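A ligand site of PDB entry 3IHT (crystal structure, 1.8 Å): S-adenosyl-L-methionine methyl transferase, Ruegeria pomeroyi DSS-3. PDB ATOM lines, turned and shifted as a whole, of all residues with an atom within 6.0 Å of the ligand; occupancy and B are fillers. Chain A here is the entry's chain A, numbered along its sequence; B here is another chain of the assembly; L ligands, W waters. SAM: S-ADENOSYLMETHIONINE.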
ATOM      1  N   GLN A  26      21.338 -18.653  25.028  1.00  0.00           N
ATOM      2  CA  GLN A  26      19.896 -18.335  25.112  1.00  0.00           C
ATOM      3  C   GLN A  26      19.031 -19.496  24.861  1.00  0.00           C
ATOM      4  O   GLN A  26      18.045 -19.720  25.580  1.00  0.00           O
ATOM      5  CB  GLN A  26      19.506 -17.260  24.085  1.00  0.00           C
ATOM      6  CG  GLN A  26      20.003 -15.927  24.417  1.00  0.00           C
ATOM      7  CD  GLN A  26      19.807 -14.920  23.278  1.00  0.00           C
ATOM      8  OE1 GLN A  26      19.846 -15.270  22.086  1.00  0.00           O
ATOM      9  NE2 GLN A  26      19.585 -13.671  23.633  1.00  0.00           N
ATOM     10  N   GLU A  46       8.929 -11.290  27.364  1.00  0.00           N
ATOM     11  CA  GLU A  46      10.080 -11.158  26.477  1.00  0.00           C
ATOM     12  C   GLU A  46      10.435  -9.681  26.398  1.00  0.00           C
ATOM     13  O   GLU A  46       9.674  -8.883  25.835  1.00  0.00           O
ATOM     14  CB  GLU A  46       9.707 -11.712  25.087  1.00  0.00           C
ATOM     15  CG  GLU A  46      10.705 -11.459  23.961  1.00  0.00           C
ATOM     16  CD  GLU A  46      11.954 -12.317  24.036  1.00  0.00           C
ATOM     17  OE1 GLU A  46      12.170 -12.965  25.085  1.00  0.00           O
ATOM     18  OE2 GLU A  46      12.712 -12.378  23.042  1.00  0.00           O
ATOM     19  N   LEU A  47      11.571  -9.311  26.985  1.00  0.00           N
ATOM     20  CA  LEU A  47      11.957  -7.900  27.043  1.00  0.00           C
ATOM     21  C   LEU A  47      12.919  -7.626  25.897  1.00  0.00           C
ATOM     22  O   LEU A  47      14.099  -8.065  25.921  1.00  0.00           O
ATOM     23  CB  LEU A  47      12.611  -7.558  28.413  1.00  0.00           C
ATOM     24  CG  LEU A  47      11.768  -7.945  29.626  1.00  0.00           C
ATOM     25  CD1 LEU A  47      12.434  -7.473  30.946  1.00  0.00           C
ATOM     26  CD2 LEU A  47      10.355  -7.378  29.524  1.00  0.00           C
ATOM     27  N   GLY A  48      12.439  -6.883  24.901  1.00  0.00           N
ATOM     28  CA  GLY A  48      13.223  -6.617  23.701  1.00  0.00           C
ATOM     29  C   GLY A  48      12.875  -7.595  22.602  1.00  0.00           C
ATOM     30  O   GLY A  48      13.169  -8.785  22.694  1.00  0.00           O
ATOM     31  N   LEU A  49      12.258  -7.123  21.556  1.00  0.00           N
ATOM     32  CA  LEU A  49      11.881  -7.998  20.439  1.00  0.00           C
ATOM     33  C   LEU A  49      12.985  -8.130  19.402  1.00  0.00           C
ATOM     34  O   LEU A  49      13.360  -9.214  19.006  1.00  0.00           O
ATOM     35  CB  LEU A  49      10.601  -7.444  19.772  1.00  0.00           C
ATOM     36  CG  LEU A  49      10.087  -8.246  18.588  1.00  0.00           C
ATOM     37  CD1 LEU A  49       9.765  -9.735  18.957  1.00  0.00           C
ATOM     38  CD2 LEU A  49       8.854  -7.527  17.958  1.00  0.00           C
ATOM     39  N   GLY A  50      13.495  -6.979  18.933  1.00  0.00           N
ATOM     40  CA  GLY A  50      14.451  -6.933  17.844  1.00  0.00           C
ATOM     41  C   GLY A  50      14.006  -7.673  16.593  1.00  0.00           C
ATOM     42  O   GLY A  50      12.846  -7.577  16.190  1.00  0.00           O
ATOM     43  N   ASN A  51      14.915  -8.438  16.006  1.00  0.00           N
ATOM     44  CA  ASN A  51      14.572  -9.244  14.830  1.00  0.00           C
ATOM     45  C   ASN A  51      13.505 -10.291  15.154  1.00  0.00           C
ATOM     46  O   ASN A  51      12.752 -10.693  14.265  1.00  0.00           O
ATOM     47  CB  ASN A  51      15.837  -9.938  14.302  1.00  0.00           C
ATOM     48  CG  ASN A  51      15.602 -10.726  13.053  1.00  0.00           C
ATOM     49  OD1 ASN A  51      15.306 -11.924  13.115  1.00  0.00           O
ATOM     50  ND2 ASN A  51      15.788 -10.086  11.897  1.00  0.00           N
ATOM     51  N   GLY A  52      13.499 -10.771  16.383  1.00  0.00           N
ATOM     52  CA  GLY A  52      12.482 -11.653  16.895  1.00  0.00           C
ATOM     53  C   GLY A  52      12.833 -13.130  16.962  1.00  0.00           C
ATOM     54  O   GLY A  52      11.941 -13.997  17.124  1.00  0.00           O
ATOM     55  N   ARG A  53      14.139 -13.472  16.897  1.00  0.00           N
ATOM     56  CA  ARG A  53      14.544 -14.884  16.945  1.00  0.00           C
ATOM     57  C   ARG A  53      14.255 -15.592  18.238  1.00  0.00           C
ATOM     58  O   ARG A  53      13.761 -16.724  18.213  1.00  0.00           O
ATOM     59  CB  ARG A  53      16.020 -15.089  16.518  1.00  0.00           C
ATOM     60  CG  ARG A  53      16.281 -14.676  15.071  1.00  0.00           C
ATOM     61  CD  ARG A  53      17.656 -15.097  14.549  1.00  0.00           C
ATOM     62  NE  ARG A  53      17.831 -14.739  13.148  1.00  0.00           N
ATOM     63  CZ  ARG A  53      18.252 -13.559  12.698  1.00  0.00           C
ATOM     64  NH1 ARG A  53      18.570 -12.567  13.525  1.00  0.00           N
ATOM     65  NH2 ARG A  53      18.338 -13.373  11.389  1.00  0.00           N
ATOM     66  N   THR A  54      14.534 -14.975  19.382  1.00  0.00           N
ATOM     67  CA  THR A  54      14.236 -15.649  20.637  1.00  0.00           C
ATOM     68  C   THR A  54      12.736 -15.676  20.844  1.00  0.00           C
ATOM     69  O   THR A  54      12.239 -16.629  21.404  1.00  0.00           O
ATOM     70  CB  THR A  54      14.929 -15.101  21.952  1.00  0.00           C
ATOM     71  OG1 THR A  54      14.771 -13.682  22.060  1.00  0.00           O
ATOM     72  CG2 THR A  54      16.441 -15.544  22.012  1.00  0.00           C
ATOM     73  N   TYR A  55      12.032 -14.641  20.415  1.00  0.00           N
ATOM     74  CA  TYR A  55      10.567 -14.672  20.496  1.00  0.00           C
ATOM     75  C   TYR A  55      10.005 -15.859  19.678  1.00  0.00           C
ATOM     76  O   TYR A  55       9.146 -16.596  20.156  1.00  0.00           O
ATOM     77  CB  TYR A  55       9.963 -13.355  20.038  1.00  0.00           C
ATOM     78  CG  TYR A  55       8.445 -13.416  19.993  1.00  0.00           C
ATOM     79  CD1 TYR A  55       7.679 -13.660  21.142  1.00  0.00           C
ATOM     80  CD2 TYR A  55       7.785 -13.167  18.800  1.00  0.00           C
ATOM     81  CE1 TYR A  55       6.241 -13.754  21.074  1.00  0.00           C
ATOM     82  CE2 TYR A  55       6.367 -13.245  18.704  1.00  0.00           C
ATOM     83  CZ  TYR A  55       5.605 -13.518  19.849  1.00  0.00           C
ATOM     84  OH  TYR A  55       4.220 -13.581  19.724  1.00  0.00           O
ATOM     85  N   PHE A  70       7.730  -6.881  25.196  1.00  0.00           N
ATOM     86  CA  PHE A  70       7.975  -5.478  25.583  1.00  0.00           C
ATOM     87  C   PHE A  70       8.972  -4.907  24.577  1.00  0.00           C
ATOM     88  O   PHE A  70      10.066  -5.458  24.384  1.00  0.00           O
ATOM     89  CB  PHE A  70       8.566  -5.392  26.979  1.00  0.00           C
ATOM     90  CG  PHE A  70       7.643  -5.822  28.084  1.00  0.00           C
ATOM     91  CD1 PHE A  70       7.280  -7.158  28.232  1.00  0.00           C
ATOM     92  CD2 PHE A  70       7.172  -4.905  29.005  1.00  0.00           C
ATOM     93  CE1 PHE A  70       6.464  -7.571  29.263  1.00  0.00           C
ATOM     94  CE2 PHE A  70       6.344  -5.315  30.055  1.00  0.00           C
ATOM     95  CZ  PHE A  70       6.002  -6.626  30.186  1.00  0.00           C
ATOM     96  N   GLU A  71       8.586  -3.872  23.869  1.00  0.00           N
ATOM     97  CA  GLU A  71       9.449  -3.312  22.823  1.00  0.00           C
ATOM     98  C   GLU A  71       9.070  -1.847  22.591  1.00  0.00           C
ATOM     99  O   GLU A  71       7.910  -1.456  22.709  1.00  0.00           O
ATOM    100  CB  GLU A  71       9.296  -4.142  21.509  1.00  0.00           C
ATOM    101  CG  GLU A  71      10.002  -3.631  20.318  1.00  0.00           C
ATOM    102  CD  GLU A  71      11.517  -3.447  20.550  1.00  0.00           C
ATOM    103  OE1 GLU A  71      12.212  -4.455  20.767  1.00  0.00           O
ATOM    104  OE2 GLU A  71      12.002  -2.307  20.493  1.00  0.00           O
ATOM    105  N   ARG A  72      10.069  -1.028  22.280  1.00  0.00           N
ATOM    106  CA  ARG A  72       9.849   0.386  22.034  1.00  0.00           C
ATOM    107  C   ARG A  72       9.522   0.636  20.577  1.00  0.00           C
ATOM    108  O   ARG A  72       8.757   1.536  20.268  1.00  0.00           O
ATOM    109  CB  ARG A  72      11.063   1.236  22.500  1.00  0.00           C
ATOM    110  CG  ARG A  72      12.333   1.044  21.711  1.00  0.00           C
ATOM    111  CD  ARG A  72      13.513   1.693  22.465  1.00  0.00           C
ATOM    112  NE  ARG A  72      14.795   1.108  22.123  1.00  0.00           N
ATOM    113  CZ  ARG A  72      15.922   1.367  22.781  1.00  0.00           C
ATOM    114  NH1 ARG A  72      15.921   2.177  23.829  1.00  0.00           N
ATOM    115  NH2 ARG A  72      17.057   0.805  22.391  1.00  0.00           N
ATOM    116  N   ALA A  73      10.083  -0.175  19.669  1.00  0.00           N
ATOM    117  CA  ALA A  73       9.823  -0.017  18.242  1.00  0.00           C
ATOM    118  C   ALA A  73       9.829  -1.376  17.522  1.00  0.00           C
ATOM    119  O   ALA A  73      10.860  -2.038  17.476  1.00  0.00           O
ATOM    120  CB  ALA A  73      10.898   0.882  17.657  1.00  0.00           C
ATOM    121  N   GLY A  90       6.463   0.517  24.279  1.00  0.00           N
ATOM    122  CA  GLY A  90       7.034   1.671  24.953  1.00  0.00           C
ATOM    123  C   GLY A  90       8.353   1.316  25.619  1.00  0.00           C
ATOM    124  O   GLY A  90       8.915   0.236  25.422  1.00  0.00           O
ATOM    125  N   ASP A  91       8.836   2.244  26.385  1.00  0.00           N
ATOM    126  CA  ASP A  91      10.096   2.073  27.080  1.00  0.00           C
ATOM    127  C   ASP A  91       9.824   1.287  28.344  1.00  0.00           C
ATOM    128  O   ASP A  91       8.982   1.700  29.150  1.00  0.00           O
ATOM    129  CB  ASP A  91      10.655   3.444  27.425  1.00  0.00           C
ATOM    130  CG  ASP A  91      12.101   3.370  27.877  1.00  0.00           C
ATOM    131  OD1 ASP A  91      12.411   2.581  28.793  1.00  0.00           O
ATOM    132  OD2 ASP A  91      12.943   4.071  27.282  1.00  0.00           O
ATOM    133  N   ILE A  92      10.552   0.192  28.536  1.00  0.00           N
ATOM    134  CA  ILE A  92      10.318  -0.675  29.692  1.00  0.00           C
ATOM    135  C   ILE A  92      10.485   0.037  31.021  1.00  0.00           C
ATOM    136  O   ILE A  92       9.941  -0.412  32.022  1.00  0.00           O
ATOM    137  CB  ILE A  92      11.110  -1.991  29.676  1.00  0.00           C
ATOM    138  CG1 ILE A  92      12.609  -1.735  29.715  1.00  0.00           C
ATOM    139  CG2 ILE A  92      10.722  -2.844  28.447  1.00  0.00           C
ATOM    140  CD1 ILE A  92      13.422  -3.042  29.877  1.00  0.00           C
ATOM    141  N   ARG A  93      11.179   1.170  31.045  1.00  0.00           N
ATOM    142  CA  ARG A  93      11.316   1.904  32.294  1.00  0.00           C
ATOM    143  C   ARG A  93       9.954   2.447  32.773  1.00  0.00           C
ATOM    144  O   ARG A  93       9.729   2.606  33.978  1.00  0.00           O
ATOM    145  CB  ARG A  93      12.415   2.973  32.163  1.00  0.00           C
ATOM    146  CG  ARG A  93      13.817   2.337  32.033  1.00  0.00           C
ATOM    147  CD  ARG A  93      14.917   3.290  31.509  1.00  0.00           C
ATOM    148  NE  ARG A  93      14.650   3.816  30.169  1.00  0.00           N
ATOM    149  CZ  ARG A  93      15.406   4.710  29.554  1.00  0.00           C
ATOM    150  NH1 ARG A  93      16.526   5.151  30.131  1.00  0.00           N
ATOM    151  NH2 ARG A  93      15.074   5.155  28.336  1.00  0.00           N
ATOM    152  N   HIS A 111      12.457 -13.027  30.241  1.00  0.00           N
ATOM    153  CA  HIS A 111      13.668 -13.122  29.426  1.00  0.00           C
ATOM    154  C   HIS A 111      14.066 -11.744  28.931  1.00  0.00           C
ATOM    155  O   HIS A 111      13.218 -11.034  28.359  1.00  0.00           O
ATOM    156  CB  HIS A 111      13.461 -14.031  28.192  1.00  0.00           C
ATOM    157  CG  HIS A 111      14.641 -14.027  27.278  1.00  0.00           C
ATOM    158  ND1 HIS A 111      14.555 -13.713  25.937  1.00  0.00           N
ATOM    159  CD2 HIS A 111      15.955 -14.283  27.525  1.00  0.00           C
ATOM    160  CE1 HIS A 111      15.785 -13.741  25.412  1.00  0.00           C
ATOM    161  NE2 HIS A 111      16.639 -14.064  26.366  1.00  0.00           N
ATOM    162  N   ASP A 113      16.993  -9.657  26.618  1.00  0.00           N
ATOM    163  CA  ASP A 113      18.141  -9.559  25.722  1.00  0.00           C
ATOM    164  C   ASP A 113      18.093  -8.113  25.159  1.00  0.00           C
ATOM    165  O   ASP A 113      17.724  -7.880  24.018  1.00  0.00           O
ATOM    166  CB  ASP A 113      18.019 -10.610  24.596  1.00  0.00           C
ATOM    167  CG  ASP A 113      19.207 -10.643  23.656  1.00  0.00           C
ATOM    168  OD1 ASP A 113      20.362 -10.340  24.090  1.00  0.00           O
ATOM    169  OD2 ASP A 113      18.987 -10.961  22.429  1.00  0.00           O
ATOM    170  N   LEU A 114      18.350  -7.164  26.044  1.00  0.00           N
ATOM    171  CA  LEU A 114      18.143  -5.743  25.790  1.00  0.00           C
ATOM    172  C   LEU A 114      19.420  -5.016  25.354  1.00  0.00           C
ATOM    173  O   LEU A 114      19.374  -3.828  24.997  1.00  0.00           O
ATOM    174  CB  LEU A 114      17.577  -5.071  27.057  1.00  0.00           C
ATOM    175  CG  LEU A 114      16.151  -5.526  27.426  1.00  0.00           C
ATOM    176  CD1 LEU A 114      15.908  -5.472  28.982  1.00  0.00           C
ATOM    177  CD2 LEU A 114      15.140  -4.684  26.644  1.00  0.00           C
ATOM    178  N   GLY A 115      20.559  -5.733  25.364  1.00  0.00           N
ATOM    179  CA  GLY A 115      21.838  -5.109  25.085  1.00  0.00           C
ATOM    180  C   GLY A 115      22.035  -4.647  23.664  1.00  0.00           C
ATOM    181  O   GLY A 115      21.501  -5.253  22.721  1.00  0.00           O
ATOM    182  N   GLY A 116      22.790  -3.562  23.510  1.00  0.00           N
ATOM    183  CA  GLY A 116      23.237  -3.093  22.215  1.00  0.00           C
ATOM    184  C   GLY A 116      24.726  -3.382  22.087  1.00  0.00           C
ATOM    185  O   GLY A 116      25.248  -4.300  22.714  1.00  0.00           O
ATOM    186  N   PHE A 125      22.499  -0.371  32.281  1.00  0.00           N
ATOM    187  CA  PHE A 125      21.069  -0.593  32.066  1.00  0.00           C
ATOM    188  C   PHE A 125      20.569  -1.806  32.844  1.00  0.00           C
ATOM    189  O   PHE A 125      19.507  -1.756  33.451  1.00  0.00           O
ATOM    190  CB  PHE A 125      20.766  -0.780  30.579  1.00  0.00           C
ATOM    191  CG  PHE A 125      19.294  -0.751  30.257  1.00  0.00           C
ATOM    192  CD1 PHE A 125      18.550   0.389  30.436  1.00  0.00           C
ATOM    193  CD2 PHE A 125      18.669  -1.885  29.775  1.00  0.00           C
ATOM    194  CE1 PHE A 125      17.191   0.434  30.145  1.00  0.00           C
ATOM    195  CE2 PHE A 125      17.286  -1.845  29.464  1.00  0.00           C
ATOM    196  CZ  PHE A 125      16.557  -0.696  29.652  1.00  0.00           C
ATOM    197  N   LEU B  16      15.836 -19.193  15.713  1.00  0.00           N
ATOM    198  CA  LEU B  16      17.051 -19.175  16.565  1.00  0.00           C
ATOM    199  C   LEU B  16      17.933 -20.390  16.206  1.00  0.00           C
ATOM    200  O   LEU B  16      19.134 -20.248  15.984  1.00  0.00           O
ATOM    201  CB  LEU B  16      16.670 -19.198  18.035  1.00  0.00           C
ATOM    202  CG  LEU B  16      17.833 -19.002  19.046  1.00  0.00           C
ATOM    203  CD1 LEU B  16      18.621 -17.717  18.786  1.00  0.00           C
ATOM    204  CD2 LEU B  16      17.287 -19.120  20.517  1.00  0.00           C
HETATM  205  N   SAM L   1      16.368 -11.282  21.589  1.00  0.00           N
HETATM  206  CA  SAM L   1      16.134 -10.678  20.231  1.00  0.00           C
HETATM  207  C   SAM L   1      16.226 -11.752  19.121  1.00  0.00           C
HETATM  208  O   SAM L   1      16.117 -11.459  17.907  1.00  0.00           O
HETATM  209  OXT SAM L   1      16.539 -12.931  19.438  1.00  0.00           O
HETATM  210  CB  SAM L   1      17.042  -9.470  19.958  1.00  0.00           C
HETATM  211  CG  SAM L   1      16.734  -8.212  20.796  1.00  0.00           C
HETATM  212  SD  SAM L   1      17.774  -6.744  20.346  1.00  0.00           S
HETATM  213  CE  SAM L   1      19.387  -7.402  20.887  1.00  0.00           C
HETATM  214  C5' SAM L   1      17.303  -5.621  21.732  1.00  0.00           C
HETATM  215  C4' SAM L   1      15.894  -5.050  21.664  1.00  0.00           C
HETATM  216  O4' SAM L   1      15.597  -4.429  22.944  1.00  0.00           O
HETATM  217  C3' SAM L   1      15.685  -3.976  20.602  1.00  0.00           C
HETATM  218  O3' SAM L   1      14.580  -4.280  19.741  1.00  0.00           O
HETATM  219  C2' SAM L   1      15.488  -2.675  21.381  1.00  0.00           C
HETATM  220  O2' SAM L   1      14.663  -1.658  20.781  1.00  0.00           O
HETATM  221  C1' SAM L   1      14.899  -3.212  22.677  1.00  0.00           C
HETATM  222  N9  SAM L   1      15.070  -2.263  23.807  1.00  0.00           N
HETATM  223  C8  SAM L   1      16.257  -1.808  24.339  1.00  0.00           C
HETATM  224  N7  SAM L   1      15.986  -0.964  25.371  1.00  0.00           N
HETATM  225  C5  SAM L   1      14.644  -0.871  25.500  1.00  0.00           C
HETATM  226  C6  SAM L   1      13.839  -0.163  26.401  1.00  0.00           C
HETATM  227  N6  SAM L   1      14.377   0.665  27.340  1.00  0.00           N
HETATM  228  N1  SAM L   1      12.469  -0.320  26.290  1.00  0.00           N
HETATM  229  C2  SAM L   1      11.874  -1.113  25.331  1.00  0.00           C
HETATM  230  N3  SAM L   1      12.688  -1.810  24.428  1.00  0.00           N
HETATM  231  C4  SAM L   1      14.040  -1.684  24.533  1.00  0.00           C
HETATM  232  O   HOH W   1      14.829 -10.706  23.659  1.00  0.00           O
HETATM  233  O   HOH W   2      18.422  -0.023  26.453  1.00  0.00           O
HETATM  234  O   HOH W   3      18.230 -12.216  16.427  1.00  0.00           O
HETATM  235  O   HOH W   4      19.320 -13.764  19.881  1.00  0.00           O
HETATM  236  O   HOH W   5      13.582  -3.371  17.484  1.00  0.00           O
HETATM  237  O   HOH W   6      19.099  -2.504  22.504  1.00  0.00           O
HETATM  238  O   HOH W   7      17.004   2.278  27.227  1.00  0.00           O
HETATM  239  O   HOH W   8      19.667  -4.162  19.895  1.00  0.00           O
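The backbone NH (N) of Gly 52 sits at hydrogen-bond distance from an oxygen (O) of the ligand (3.1 Å). The backbone NH (N) of Thr 54 lies within hydrogen-bond range of an oxygen (OXT) of the ligand, at 2.9 Å. The backbone NH (N) of Arg 53 is in hydrogen-bond range of an oxygen (O) of the ligand. O3' of the ligand lies within hydrogen-bond range of N of Gly 50. The side-chain hydroxyl (OG1) of Thr 54 is in hydrogen-bond range of a nitrogen (N) of the ligand (2.9 Å). The backbone NH of Arg 72 is in hydrogen-bond range of a nitrogen (N3) of the ligand (3.5 Å). A nitrogen (N6) of the ligand is in hydrogen-bond range of the side-chain carboxylate of Asp 91 (3.1 Å). The side-chain carboxylate (OE1) of Glu 71 sits at hydrogen-bond distance from an oxygen (O3') of the ligand, 2.6 Å away. The backbone NH of Ile 92 sits at hydrogen-bond distance from a nitrogen (N1) of the ligand (3.0 Å). NE of Arg 72 sits at hydrogen-bond distance from O2' of the ligand (3.1 Å). A nitrogen (N) of the ligand lies within salt-bridge range of the side-chain carboxylate (OD2) of Asp 113 (2.8 Å).
Gly 48 touches the ligand. Leu 49 touches the ligand (O to CA, 3.4 Å). Asn 51 touches the ligand. O of Gly 90 touches C2 of the ligand, 3.3 Å away. Leu 114 touches the ligand. Gly 115 touches the ligand. Phe 125 touches the ligand. Hydrophobic or aromatic side chains within 4 Å of the ligand: Ile 92, Leu 114 and Phe 125. Within 4 Å of the ligand: Gly 48, Leu 49, Gly 50, Asn 51, Gly 52, Arg 53, Thr 54, Glu 71, Arg 72, Gly 90, Asp 91, Ile 92, Asp 113, Leu 114, Gly 115 and Phe 125. The nearest printed residue that does not touch the ligand is Glu 46 (4.1 Å).
Water W5 bridges an oxygen (O3') of the ligand (2.6 Å) and the backbone carbonyl oxygen (O) of Ala 73 (3.0 Å). Water W1 lies within hydrogen-bond range of a nitrogen (N) of the ligand (2.6 Å), the backbone carbonyl oxygen of Gly 48 (2.7 Å), the side-chain carboxylate of Glu 46 (2.8 Å) and the side-chain hydroxyl of Thr 54 (3.4 Å). Water W3 lies within hydrogen-bond range of an oxygen (O) of the ligand and the guanidinium group (NH1) of Arg 53. Water W4 lies within hydrogen-bond range of the side-chain amide oxygen (OE1) of Gln 26 (2.7 Å) and an oxygen (OXT) of the ligand (2.9 Å).
OD2 of Asp 91 lies within salt-bridge range of NH2 of Arg 93, at 2.6 Å. The backbone NH (N) of Asp 113 sits at hydrogen-bond distance from the backbone carbonyl oxygen (O) of Leu 47, 3.4 Å away. The guanidinium group (NH1) of Arg 53 is in hydrogen-bond range of the side-chain amide oxygen (OD1) of Asn 51, at 3.4 Å. The backbone NH (N) of Gly 50 sits at hydrogen-bond distance from the side-chain carboxylate (OE1) of Glu 71, 3.4 Å away. OE2 of Glu 46 sits at hydrogen-bond distance from OG1 of Thr 54, at 2.6 Å. The backbone NH (N) of Ala 73 lies within hydrogen-bond range of the side-chain carboxylate (OE2) of Glu 71 (3.0 Å). The side-chain carboxylate of Asp 113 is in hydrogen-bond range of the side-chain amide nitrogen of Gln 26 (3.0 Å). The side-chain carboxylate of Glu 71 lies within hydrogen-bond range of the backbone NH of Leu 49 (2.8 Å).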
